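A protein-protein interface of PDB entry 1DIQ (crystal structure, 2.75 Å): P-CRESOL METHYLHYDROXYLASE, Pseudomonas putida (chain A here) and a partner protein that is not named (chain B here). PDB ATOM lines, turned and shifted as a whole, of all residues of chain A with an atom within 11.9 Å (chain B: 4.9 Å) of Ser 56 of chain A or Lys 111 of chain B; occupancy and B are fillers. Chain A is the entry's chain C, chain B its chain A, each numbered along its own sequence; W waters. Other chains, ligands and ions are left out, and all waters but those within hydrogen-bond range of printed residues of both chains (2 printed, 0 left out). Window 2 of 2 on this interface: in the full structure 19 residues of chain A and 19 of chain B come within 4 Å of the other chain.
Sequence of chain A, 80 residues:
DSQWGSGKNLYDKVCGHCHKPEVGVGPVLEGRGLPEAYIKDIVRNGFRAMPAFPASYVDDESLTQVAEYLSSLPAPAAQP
The side-chain hydroxyl (OG) of Ser 56 of chain A is in hydrogen-bond range of the side-chain carboxylate (OD1) of Asp 109 of chain B (2.6 Å).
NZ of Lys 111 of chain B lies within hydrogen-bond range of O of Gly 131 of chain B (2.8 Å). OD1 of Asp 109 of chain B is in hydrogen-bond range of OH of Tyr 44 of chain B, 2.7 Å away. NE2 of Gln 3 of chain A lies within hydrogen-bond range of O of Ser 56 of chain A, at 3.2 Å. The side-chain carboxylate (OD2) of Asp 109 of chain B lies within hydrogen-bond range of the backbone NH (N) of Lys 111 of chain B. The backbone carbonyl oxygen (O) of Tyr 57 of chain A sits close to the side-chain amide oxygen (OE1) of Gln 3 of chain A (3.2 Å). The backbone NH (N) of Lys 111 of chain B sits close to the backbone carbonyl oxygen (O) of Ser 88 of chain B (3.5 Å).
Pro 54 of chain A touches Tyr 44 of chain B (CB to CZ, 3.8 Å). Tyr 44 of chain B touches Ser 56 of chain A (OH to OG, 3.9 Å). Ser 56 of chain A touches Lys 111 of chain B. Lys 111 of chain B touches Tyr 57 of chain A (CE to CD2, 3.8 Å). Tyr 57 of chain A touches Thr 133 of chain B (OH to CG2, 3.4 Å).
Of chain B, only Tyr 44 (3.9 Å), Asp 109 (2.6 Å) and Lys 111 (3.6 Å) come within 4 Å of Ser 56 of chain A. Of the printed residues of chain B, Tyr 57 of chain A touches Lys 111 and Thr 133. Asp 59 of chain A touches none of the printed residues of chain B. Of the printed residues of chain A, Tyr 44 of chain B touches Pro 54 and Ser 56. No residue of chain A comes within 4 Å of Ser 88 of chain B. No residue of chain A comes within 4 Å of Thr 89 of chain B. Asp 109 of chain B touches one residue of chain A. No residue of chain A comes within 4 Å of Leu 110 of chain B. No residue of chain A comes within 4 Å of Lys 112 of chain B. No residue of chain A comes within 4 Å of Asn 114 of chain B. Of the printed residues of chain A, Thr 133 of chain B touches Tyr 57 (3.4 Å). The nearest residue of chain B that does not touch Ser 56 of chain A is Lys 112 of chain B (4.1 Å). The nearest printed residue of chain B that does not touch Pro 54 of chain A is Asp 109 of chain B (4.6 Å).
Among the printed residues, no Asp or Glu carboxylate lies within 4 Å of a Lys or Arg side-chain nitrogen of the other chain.
Water W2 bridges NZ of Lys 111 of chain B (2.8 Å) and O of Ser 56 of chain A (2.9 Å). Water W1 lies within hydrogen-bond range of OH of Tyr 44 of chain B, N of Ala 55 of chain A and N of Ser 56 of chain A.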
ATOM      1  N   SER A   2     -33.867  13.760 -15.926  1.00  0.00           N
ATOM      2  CA  SER A   2     -33.562  14.591 -17.127  1.00  0.00           C
ATOM      3  C   SER A   2     -33.172  13.704 -18.332  1.00  0.00           C
ATOM      4  O   SER A   2     -33.669  12.576 -18.465  1.00  0.00           O
ATOM      5  CB  SER A   2     -32.455  15.607 -16.785  1.00  0.00           C
ATOM      6  OG  SER A   2     -31.256  14.966 -16.375  1.00  0.00           O
ATOM      7  N   GLN A   3     -32.286  14.221 -19.192  1.00  0.00           N
ATOM      8  CA  GLN A   3     -31.800  13.530 -20.387  1.00  0.00           C
ATOM      9  C   GLN A   3     -30.859  12.385 -20.019  1.00  0.00           C
ATOM     10  O   GLN A   3     -30.883  11.331 -20.656  1.00  0.00           O
ATOM     11  CB  GLN A   3     -31.084  14.526 -21.294  1.00  0.00           C
ATOM     12  CG  GLN A   3     -30.773  14.036 -22.707  1.00  0.00           C
ATOM     13  CD  GLN A   3     -29.840  14.976 -23.436  1.00  0.00           C
ATOM     14  OE1 GLN A   3     -28.809  15.376 -22.899  1.00  0.00           O
ATOM     15  NE2 GLN A   3     -30.205  15.356 -24.657  1.00  0.00           N
ATOM     16  N   TRP A   4     -30.027  12.608 -19.001  1.00  0.00           N
ATOM     17  CA  TRP A   4     -29.086  11.592 -18.520  1.00  0.00           C
ATOM     18  C   TRP A   4     -29.445  11.104 -17.113  1.00  0.00           C
ATOM     19  O   TRP A   4     -28.808  10.188 -16.582  1.00  0.00           O
ATOM     20  CB  TRP A   4     -27.640  12.106 -18.586  1.00  0.00           C
ATOM     21  CG  TRP A   4     -27.131  12.261 -20.004  1.00  0.00           C
ATOM     22  CD1 TRP A   4     -27.183  13.393 -20.781  1.00  0.00           C
ATOM     23  CD2 TRP A   4     -26.556  11.240 -20.826  1.00  0.00           C
ATOM     24  NE1 TRP A   4     -26.683  13.138 -22.033  1.00  0.00           N
ATOM     25  CE2 TRP A   4     -26.288  11.828 -22.097  1.00  0.00           C
ATOM     26  CE3 TRP A   4     -26.240   9.878 -20.622  1.00  0.00           C
ATOM     27  CZ2 TRP A   4     -25.720  11.102 -23.162  1.00  0.00           C
ATOM     28  CZ3 TRP A   4     -25.675   9.151 -21.681  1.00  0.00           C
ATOM     29  CH2 TRP A   4     -25.422   9.772 -22.938  1.00  0.00           C
ATOM     30  N   GLY A   5     -30.505  11.696 -16.547  1.00  0.00           N
ATOM     31  CA  GLY A   5     -30.989  11.339 -15.221  1.00  0.00           C
ATOM     32  C   GLY A   5     -30.258  12.040 -14.088  1.00  0.00           C
ATOM     33  O   GLY A   5     -30.840  12.837 -13.328  1.00  0.00           O
ATOM     34  N   ASN A   9     -24.392   9.576 -13.960  1.00  0.00           N
ATOM     35  CA  ASN A   9     -24.713   8.784 -15.131  1.00  0.00           C
ATOM     36  C   ASN A   9     -24.066   9.356 -16.399  1.00  0.00           C
ATOM     37  O   ASN A   9     -23.512   8.599 -17.200  1.00  0.00           O
ATOM     38  CB  ASN A   9     -26.230   8.621 -15.269  1.00  0.00           C
ATOM     39  CG  ASN A   9     -26.602   7.483 -16.192  1.00  0.00           C
ATOM     40  OD1 ASN A   9     -26.224   6.336 -15.950  1.00  0.00           O
ATOM     41  ND2 ASN A   9     -27.290   7.799 -17.292  1.00  0.00           N
ATOM     42  N   LEU A  10     -24.062  10.686 -16.536  1.00  0.00           N
ATOM     43  CA  LEU A  10     -23.430  11.327 -17.692  1.00  0.00           C
ATOM     44  C   LEU A  10     -21.939  11.038 -17.661  1.00  0.00           C
ATOM     45  O   LEU A  10     -21.371  10.638 -18.669  1.00  0.00           O
ATOM     46  CB  LEU A  10     -23.660  12.847 -17.708  1.00  0.00           C
ATOM     47  CG  LEU A  10     -22.937  13.671 -18.789  1.00  0.00           C
ATOM     48  CD1 LEU A  10     -23.294  13.207 -20.204  1.00  0.00           C
ATOM     49  CD2 LEU A  10     -23.287  15.113 -18.616  1.00  0.00           C
ATOM     50  N   LYS A  13     -21.310   7.154 -18.501  1.00  0.00           N
ATOM     51  CA  LYS A  13     -21.619   6.796 -19.879  1.00  0.00           C
ATOM     52  C   LYS A  13     -20.861   7.557 -20.976  1.00  0.00           C
ATOM     53  O   LYS A  13     -20.695   7.031 -22.075  1.00  0.00           O
ATOM     54  CB  LYS A  13     -23.137   6.880 -20.143  1.00  0.00           C
ATOM     55  CG  LYS A  13     -24.060   6.149 -19.163  1.00  0.00           C
ATOM     56  CD  LYS A  13     -23.773   4.671 -19.027  1.00  0.00           C
ATOM     57  CE  LYS A  13     -24.804   4.015 -18.113  1.00  0.00           C
ATOM     58  NZ  LYS A  13     -24.516   2.563 -17.922  1.00  0.00           N
ATOM     59  N   VAL A  14     -20.451   8.797 -20.714  1.00  0.00           N
ATOM     60  CA  VAL A  14     -19.748   9.584 -21.728  1.00  0.00           C
ATOM     61  C   VAL A  14     -18.370  10.096 -21.318  1.00  0.00           C
ATOM     62  O   VAL A  14     -17.357   9.572 -21.794  1.00  0.00           O
ATOM     63  CB  VAL A  14     -20.592  10.793 -22.231  1.00  0.00           C
ATOM     64  CG1 VAL A  14     -19.852  11.557 -23.331  1.00  0.00           C
ATOM     65  CG2 VAL A  14     -21.902  10.339 -22.750  1.00  0.00           C
ATOM     66  N   LYS A  40     -19.199  24.073 -19.071  1.00  0.00           N
ATOM     67  CA  LYS A  40     -20.194  24.387 -20.094  1.00  0.00           C
ATOM     68  C   LYS A  40     -19.509  24.948 -21.345  1.00  0.00           C
ATOM     69  O   LYS A  40     -19.960  24.699 -22.445  1.00  0.00           O
ATOM     70  CB  LYS A  40     -21.164  25.426 -19.545  1.00  0.00           C
ATOM     71  CG  LYS A  40     -22.624  25.197 -19.831  1.00  0.00           C
ATOM     72  CD  LYS A  40     -23.452  25.828 -18.705  1.00  0.00           C
ATOM     73  CE  LYS A  40     -24.949  25.546 -18.843  1.00  0.00           C
ATOM     74  NZ  LYS A  40     -25.735  26.047 -17.669  1.00  0.00           N
ATOM     75  N   VAL A  43     -17.337  21.897 -23.142  1.00  0.00           N
ATOM     76  CA  VAL A  43     -18.192  20.906 -23.794  1.00  0.00           C
ATOM     77  C   VAL A  43     -18.890  21.480 -25.016  1.00  0.00           C
ATOM     78  O   VAL A  43     -18.995  20.810 -26.036  1.00  0.00           O
ATOM     79  CB  VAL A  43     -19.161  20.250 -22.799  1.00  0.00           C
ATOM     80  CG1 VAL A  43     -20.094  19.253 -23.466  1.00  0.00           C
ATOM     81  CG2 VAL A  43     -18.372  19.506 -21.806  1.00  0.00           C
ATOM     82  N   ARG A  44     -19.273  22.746 -24.957  1.00  0.00           N
ATOM     83  CA  ARG A  44     -19.930  23.365 -26.100  1.00  0.00           C
ATOM     84  C   ARG A  44     -18.960  23.799 -27.186  1.00  0.00           C
ATOM     85  O   ARG A  44     -19.292  23.702 -28.346  1.00  0.00           O
ATOM     86  CB  ARG A  44     -20.824  24.531 -25.670  1.00  0.00           C
ATOM     87  CG  ARG A  44     -22.066  24.115 -24.881  1.00  0.00           C
ATOM     88  CD  ARG A  44     -23.141  23.490 -25.763  1.00  0.00           C
ATOM     89  NE  ARG A  44     -24.339  23.170 -24.993  1.00  0.00           N
ATOM     90  CZ  ARG A  44     -24.605  21.978 -24.473  1.00  0.00           C
ATOM     91  NH1 ARG A  44     -23.769  20.960 -24.645  1.00  0.00           N
ATOM     92  NH2 ARG A  44     -25.692  21.815 -23.734  1.00  0.00           N
ATOM     93  N   ALA A  52     -16.518  18.484 -29.236  1.00  0.00           N
ATOM     94  CA  ALA A  52     -17.613  19.299 -28.715  1.00  0.00           C
ATOM     95  C   ALA A  52     -18.871  18.466 -28.820  1.00  0.00           C
ATOM     96  O   ALA A  52     -18.992  17.641 -29.727  1.00  0.00           O
ATOM     97  CB  ALA A  52     -17.760  20.538 -29.518  1.00  0.00           C
ATOM     98  N   PHE A  53     -19.756  18.599 -27.842  1.00  0.00           N
ATOM     99  CA  PHE A  53     -21.016  17.869 -27.850  1.00  0.00           C
ATOM    100  C   PHE A  53     -22.160  18.857 -27.926  1.00  0.00           C
ATOM    101  O   PHE A  53     -22.197  19.817 -27.143  1.00  0.00           O
ATOM    102  CB  PHE A  53     -21.187  17.041 -26.588  1.00  0.00           C
ATOM    103  CG  PHE A  53     -20.195  15.953 -26.441  1.00  0.00           C
ATOM    104  CD1 PHE A  53     -18.943  16.204 -25.859  1.00  0.00           C
ATOM    105  CD2 PHE A  53     -20.514  14.651 -26.832  1.00  0.00           C
ATOM    106  CE1 PHE A  53     -18.013  15.161 -25.662  1.00  0.00           C
ATOM    107  CE2 PHE A  53     -19.597  13.595 -26.642  1.00  0.00           C
ATOM    108  CZ  PHE A  53     -18.343  13.853 -26.054  1.00  0.00           C
ATOM    109  N   PRO A  54     -23.078  18.684 -28.900  1.00  0.00           N
ATOM    110  CA  PRO A  54     -24.222  19.602 -29.019  1.00  0.00           C
ATOM    111  C   PRO A  54     -25.242  19.375 -27.896  1.00  0.00           C
ATOM    112  O   PRO A  54     -25.174  18.358 -27.191  1.00  0.00           O
ATOM    113  CB  PRO A  54     -24.790  19.265 -30.394  1.00  0.00           C
ATOM    114  CG  PRO A  54     -23.598  18.771 -31.139  1.00  0.00           C
ATOM    115  CD  PRO A  54     -22.951  17.877 -30.125  1.00  0.00           C
ATOM    116  N   ALA A  55     -26.171  20.322 -27.723  1.00  0.00           N
ATOM    117  CA  ALA A  55     -27.206  20.235 -26.684  1.00  0.00           C
ATOM    118  C   ALA A  55     -28.076  18.989 -26.835  1.00  0.00           C
ATOM    119  O   ALA A  55     -28.455  18.369 -25.830  1.00  0.00           O
ATOM    120  CB  ALA A  55     -28.053  21.489 -26.670  1.00  0.00           C
ATOM    121  N   SER A  56     -28.261  18.564 -28.094  1.00  0.00           N
ATOM    122  CA  SER A  56     -29.043  17.377 -28.432  1.00  0.00           C
ATOM    123  C   SER A  56     -28.415  16.086 -27.897  1.00  0.00           C
ATOM    124  O   SER A  56     -29.106  15.091 -27.683  1.00  0.00           O
ATOM    125  CB  SER A  56     -29.221  17.282 -29.929  1.00  0.00           C
ATOM    126  OG  SER A  56     -27.956  17.261 -30.549  1.00  0.00           O
ATOM    127  N   TYR A  57     -27.106  16.126 -27.668  1.00  0.00           N
ATOM    128  CA  TYR A  57     -26.379  14.981 -27.146  1.00  0.00           C
ATOM    129  C   TYR A  57     -26.312  15.092 -25.630  1.00  0.00           C
ATOM    130  O   TYR A  57     -26.630  14.132 -24.934  1.00  0.00           O
ATOM    131  CB  TYR A  57     -24.965  14.910 -27.755  1.00  0.00           C
ATOM    132  CG  TYR A  57     -24.325  13.523 -27.759  1.00  0.00           C
ATOM    133  CD1 TYR A  57     -24.135  12.805 -26.559  1.00  0.00           C
ATOM    134  CD2 TYR A  57     -23.919  12.920 -28.969  1.00  0.00           C
ATOM    135  CE1 TYR A  57     -23.576  11.531 -26.549  1.00  0.00           C
ATOM    136  CE2 TYR A  57     -23.348  11.635 -28.977  1.00  0.00           C
ATOM    137  CZ  TYR A  57     -23.187  10.950 -27.752  1.00  0.00           C
ATOM    138  OH  TYR A  57     -22.686   9.683 -27.706  1.00  0.00           O
ATOM    139  N   VAL A  58     -25.808  16.228 -25.140  1.00  0.00           N
ATOM    140  CA  VAL A  58     -25.679  16.511 -23.701  1.00  0.00           C
ATOM    141  C   VAL A  58     -26.269  17.909 -23.485  1.00  0.00           C
ATOM    142  O   VAL A  58     -25.653  18.894 -23.906  1.00  0.00           O
ATOM    143  CB  VAL A  58     -24.171  16.507 -23.224  1.00  0.00           C
ATOM    144  CG1 VAL A  58     -24.078  16.687 -21.743  1.00  0.00           C
ATOM    145  CG2 VAL A  58     -23.475  15.223 -23.576  1.00  0.00           C
ATOM    146  N   ASP A  59     -27.449  17.993 -22.847  1.00  0.00           N
ATOM    147  CA  ASP A  59     -28.112  19.291 -22.586  1.00  0.00           C
ATOM    148  C   ASP A  59     -27.584  20.118 -21.397  1.00  0.00           C
ATOM    149  O   ASP A  59     -26.842  19.596 -20.550  1.00  0.00           O
ATOM    150  CB  ASP A  59     -29.655  19.162 -22.555  1.00  0.00           C
ATOM    151  CG  ASP A  59     -30.188  18.340 -21.374  1.00  0.00           C
ATOM    152  OD1 ASP A  59     -29.397  17.836 -20.548  1.00  0.00           O
ATOM    153  OD2 ASP A  59     -31.434  18.202 -21.277  1.00  0.00           O
ATOM    154  N   ASP A  60     -27.977  21.398 -21.351  1.00  0.00           N
ATOM    155  CA  ASP A  60     -27.564  22.353 -20.302  1.00  0.00           C
ATOM    156  C   ASP A  60     -27.802  21.847 -18.877  1.00  0.00           C
ATOM    157  O   ASP A  60     -26.915  21.927 -18.027  1.00  0.00           O
ATOM    158  CB  ASP A  60     -28.237  23.728 -20.492  1.00  0.00           C
ATOM    159  CG  ASP A  60     -27.697  24.512 -21.706  1.00  0.00           C
ATOM    160  OD1 ASP A  60     -28.308  25.545 -22.074  1.00  0.00           O
ATOM    161  OD2 ASP A  60     -26.666  24.120 -22.295  1.00  0.00           O
ATOM    162  N   GLU A  61     -28.952  21.215 -18.668  1.00  0.00           N
ATOM    163  CA  GLU A  61     -29.336  20.678 -17.374  1.00  0.00           C
ATOM    164  C   GLU A  61     -28.390  19.561 -16.917  1.00  0.00           C
ATOM    165  O   GLU A  61     -28.042  19.478 -15.735  1.00  0.00           O
ATOM    166  CB  GLU A  61     -30.778  20.168 -17.454  1.00  0.00           C
ATOM    167  CG  GLU A  61     -31.528  20.120 -16.127  1.00  0.00           C
ATOM    168  CD  GLU A  61     -33.013  19.841 -16.307  1.00  0.00           C
ATOM    169  OE1 GLU A  61     -33.746  20.753 -16.764  1.00  0.00           O
ATOM    170  OE2 GLU A  61     -33.446  18.709 -15.994  1.00  0.00           O
ATOM    171  N   SER A  62     -27.925  18.762 -17.881  1.00  0.00           N
ATOM    172  CA  SER A  62     -27.023  17.636 -17.628  1.00  0.00           C
ATOM    173  C   SER A  62     -25.600  18.091 -17.337  1.00  0.00           C
ATOM    174  O   SER A  62     -24.851  17.410 -16.613  1.00  0.00           O
ATOM    175  CB  SER A  62     -27.035  16.674 -18.816  1.00  0.00           C
ATOM    176  OG  SER A  62     -28.330  16.132 -19.021  1.00  0.00           O
ATOM    177  N   LEU A  63     -25.234  19.241 -17.910  1.00  0.00           N
ATOM    178  CA  LEU A  63     -23.917  19.828 -17.693  1.00  0.00           C
ATOM    179  C   LEU A  63     -23.815  20.363 -16.260  1.00  0.00           C
ATOM    180  O   LEU A  63     -22.782  20.188 -15.602  1.00  0.00           O
ATOM    181  CB  LEU A  63     -23.638  20.936 -18.713  1.00  0.00           C
ATOM    182  CG  LEU A  63     -23.224  20.452 -20.107  1.00  0.00           C
ATOM    183  CD1 LEU A  63     -23.098  21.633 -21.061  1.00  0.00           C
ATOM    184  CD2 LEU A  63     -21.911  19.659 -20.032  1.00  0.00           C
ATOM    185  N   TYR B  44     -21.238  22.269 -33.323  1.00  0.00           N
ATOM    186  CA  TYR B  44     -21.332  21.566 -34.597  1.00  0.00           C
ATOM    187  C   TYR B  44     -20.158  21.933 -35.518  1.00  0.00           C
ATOM    188  O   TYR B  44     -19.826  21.192 -36.447  1.00  0.00           O
ATOM    189  CB  TYR B  44     -22.623  21.950 -35.305  1.00  0.00           C
ATOM    190  CG  TYR B  44     -23.895  21.485 -34.646  1.00  0.00           C
ATOM    191  CD1 TYR B  44     -24.335  20.153 -34.767  1.00  0.00           C
ATOM    192  CD2 TYR B  44     -24.708  22.392 -33.951  1.00  0.00           C
ATOM    193  CE1 TYR B  44     -25.575  19.739 -34.212  1.00  0.00           C
ATOM    194  CE2 TYR B  44     -25.943  21.996 -33.385  1.00  0.00           C
ATOM    195  CZ  TYR B  44     -26.368  20.674 -33.519  1.00  0.00           C
ATOM    196  OH  TYR B  44     -27.553  20.297 -32.935  1.00  0.00           O
ATOM    197  N   THR B  63     -33.596  19.877 -35.107  1.00  0.00           N
ATOM    198  CA  THR B  63     -33.654  18.551 -34.509  1.00  0.00           C
ATOM    199  C   THR B  63     -35.036  17.886 -34.620  1.00  0.00           C
ATOM    200  O   THR B  63     -35.990  18.272 -33.940  1.00  0.00           O
ATOM    201  CB  THR B  63     -33.155  18.547 -33.029  1.00  0.00           C
ATOM    202  OG1 THR B  63     -33.868  19.518 -32.269  1.00  0.00           O
ATOM    203  CG2 THR B  63     -31.674  18.859 -32.947  1.00  0.00           C
ATOM    204  N   ILE B  87     -26.813  14.447 -40.060  1.00  0.00           N
ATOM    205  CA  ILE B  87     -25.903  13.759 -39.153  1.00  0.00           C
ATOM    206  C   ILE B  87     -26.760  12.892 -38.194  1.00  0.00           C
ATOM    207  O   ILE B  87     -27.933  13.200 -37.956  1.00  0.00           O
ATOM    208  CB  ILE B  87     -24.964  14.721 -38.364  1.00  0.00           C
ATOM    209  CG1 ILE B  87     -25.748  15.666 -37.450  1.00  0.00           C
ATOM    210  CG2 ILE B  87     -24.045  15.454 -39.313  1.00  0.00           C
ATOM    211  CD1 ILE B  87     -24.897  16.361 -36.391  1.00  0.00           C
ATOM    212  N   SER B  88     -26.199  11.791 -37.695  1.00  0.00           N
ATOM    213  CA  SER B  88     -26.932  10.906 -36.787  1.00  0.00           C
ATOM    214  C   SER B  88     -26.400  11.097 -35.394  1.00  0.00           C
ATOM    215  O   SER B  88     -27.078  11.677 -34.559  1.00  0.00           O
ATOM    216  CB  SER B  88     -26.797   9.462 -37.230  1.00  0.00           C
ATOM    217  OG  SER B  88     -27.507   9.258 -38.440  1.00  0.00           O
ATOM    218  N   THR B  89     -25.195  10.596 -35.139  1.00  0.00           N
ATOM    219  CA  THR B  89     -24.541  10.782 -33.843  1.00  0.00           C
ATOM    220  C   THR B  89     -23.423  11.833 -33.991  1.00  0.00           C
ATOM    221  O   THR B  89     -22.927  12.363 -33.002  1.00  0.00           O
ATOM    222  CB  THR B  89     -24.064   9.447 -33.210  1.00  0.00           C
ATOM    223  OG1 THR B  89     -23.552   8.567 -34.216  1.00  0.00           O
ATOM    224  CG2 THR B  89     -25.216   8.768 -32.531  1.00  0.00           C
ATOM    225  N   ASP B 109     -30.008  17.535 -37.511  1.00  0.00           N
ATOM    226  CA  ASP B 109     -29.442  16.750 -36.420  1.00  0.00           C
ATOM    227  C   ASP B 109     -30.472  15.761 -35.883  1.00  0.00           C
ATOM    228  O   ASP B 109     -31.444  16.137 -35.223  1.00  0.00           O
ATOM    229  CB  ASP B 109     -28.920  17.697 -35.330  1.00  0.00           C
ATOM    230  CG  ASP B 109     -28.392  16.971 -34.097  1.00  0.00           C
ATOM    231  OD1 ASP B 109     -28.066  17.669 -33.122  1.00  0.00           O
ATOM    232  OD2 ASP B 109     -28.297  15.729 -34.088  1.00  0.00           O
ATOM    233  N   LEU B 110     -30.203  14.483 -36.125  1.00  0.00           N
ATOM    234  CA  LEU B 110     -31.104  13.413 -35.710  1.00  0.00           C
ATOM    235  C   LEU B 110     -30.680  12.659 -34.453  1.00  0.00           C
ATOM    236  O   LEU B 110     -31.053  11.486 -34.286  1.00  0.00           O
ATOM    237  CB  LEU B 110     -31.313  12.420 -36.868  1.00  0.00           C
ATOM    238  CG  LEU B 110     -31.792  12.965 -38.209  1.00  0.00           C
ATOM    239  CD1 LEU B 110     -31.837  11.861 -39.222  1.00  0.00           C
ATOM    240  CD2 LEU B 110     -33.154  13.620 -38.041  1.00  0.00           C
ATOM    241  N   LYS B 111     -29.966  13.332 -33.546  1.00  0.00           N
ATOM    242  CA  LYS B 111     -29.508  12.674 -32.332  1.00  0.00           C
ATOM    243  C   LYS B 111     -30.649  12.336 -31.384  1.00  0.00           C
ATOM    244  O   LYS B 111     -30.591  11.308 -30.695  1.00  0.00           O
ATOM    245  CB  LYS B 111     -28.420  13.492 -31.620  1.00  0.00           C
ATOM    246  CG  LYS B 111     -27.905  12.883 -30.284  1.00  0.00           C
ATOM    247  CD  LYS B 111     -27.174  11.549 -30.458  1.00  0.00           C
ATOM    248  CE  LYS B 111     -27.085  10.792 -29.156  1.00  0.00           C
ATOM    249  NZ  LYS B 111     -28.396  10.235 -28.727  1.00  0.00           N
ATOM    250  N   LYS B 112     -31.699  13.165 -31.414  1.00  0.00           N
ATOM    251  CA  LYS B 112     -32.873  13.001 -30.556  1.00  0.00           C
ATOM    252  C   LYS B 112     -33.769  11.798 -30.932  1.00  0.00           C
ATOM    253  O   LYS B 112     -34.602  11.371 -30.123  1.00  0.00           O
ATOM    254  CB  LYS B 112     -33.663  14.303 -30.506  1.00  0.00           C
ATOM    255  CG  LYS B 112     -32.945  15.477 -29.848  1.00  0.00           C
ATOM    256  CD  LYS B 112     -33.351  15.631 -28.380  1.00  0.00           C
ATOM    257  CE  LYS B 112     -33.616  17.109 -27.994  1.00  0.00           C
ATOM    258  NZ  LYS B 112     -34.773  17.754 -28.706  1.00  0.00           N
ATOM    259  N   MET B 113     -33.586  11.272 -32.154  1.00  0.00           N
ATOM    260  CA  MET B 113     -34.282  10.075 -32.655  1.00  0.00           C
ATOM    261  C   MET B 113     -33.470   8.892 -32.118  1.00  0.00           C
ATOM    262  O   MET B 113     -32.788   8.220 -32.885  1.00  0.00           O
ATOM    263  CB  MET B 113     -34.209   9.994 -34.182  1.00  0.00           C
ATOM    264  CG  MET B 113     -35.216  10.754 -34.953  1.00  0.00           C
ATOM    265  SD  MET B 113     -35.789   9.856 -36.388  1.00  0.00           S
ATOM    266  CE  MET B 113     -35.498  10.966 -37.578  1.00  0.00           C
ATOM    267  N   ASN B 114     -33.545   8.632 -30.816  1.00  0.00           N
ATOM    268  CA  ASN B 114     -32.742   7.584 -30.209  1.00  0.00           C
ATOM    269  C   ASN B 114     -33.467   6.328 -29.726  1.00  0.00           C
ATOM    270  O   ASN B 114     -33.065   5.706 -28.736  1.00  0.00           O
ATOM    271  CB  ASN B 114     -31.872   8.206 -29.101  1.00  0.00           C
ATOM    272  CG  ASN B 114     -32.681   8.694 -27.903  1.00  0.00           C
ATOM    273  OD1 ASN B 114     -32.174   8.716 -26.780  1.00  0.00           O
ATOM    274  ND2 ASN B 114     -33.938   9.056 -28.129  1.00  0.00           N
ATOM    275  N   GLY B 131     -30.215   8.238 -33.893  1.00  0.00           N
ATOM    276  CA  GLY B 131     -29.588   8.739 -32.689  1.00  0.00           C
ATOM    277  C   GLY B 131     -29.132   7.737 -31.665  1.00  0.00           C
ATOM    278  O   GLY B 131     -28.617   8.127 -30.621  1.00  0.00           O
ATOM    279  N   THR B 133     -26.829   5.244 -29.794  1.00  0.00           N
ATOM    280  CA  THR B 133     -25.381   5.098 -29.688  1.00  0.00           C
ATOM    281  C   THR B 133     -25.070   3.656 -29.366  1.00  0.00           C
ATOM    282  O   THR B 133     -25.959   2.924 -28.919  1.00  0.00           O
ATOM    283  CB  THR B 133     -24.738   5.978 -28.597  1.00  0.00           C
ATOM    284  OG1 THR B 133     -25.187   5.563 -27.304  1.00  0.00           O
ATOM    285  CG2 THR B 133     -25.009   7.466 -28.845  1.00  0.00           C
HETATM  286  O   HOH W   1     -28.033  21.041 -30.241  1.00  0.00           O
HETATM  287  O   HOH W   2     -29.879  12.280 -27.479  1.00  0.00           O
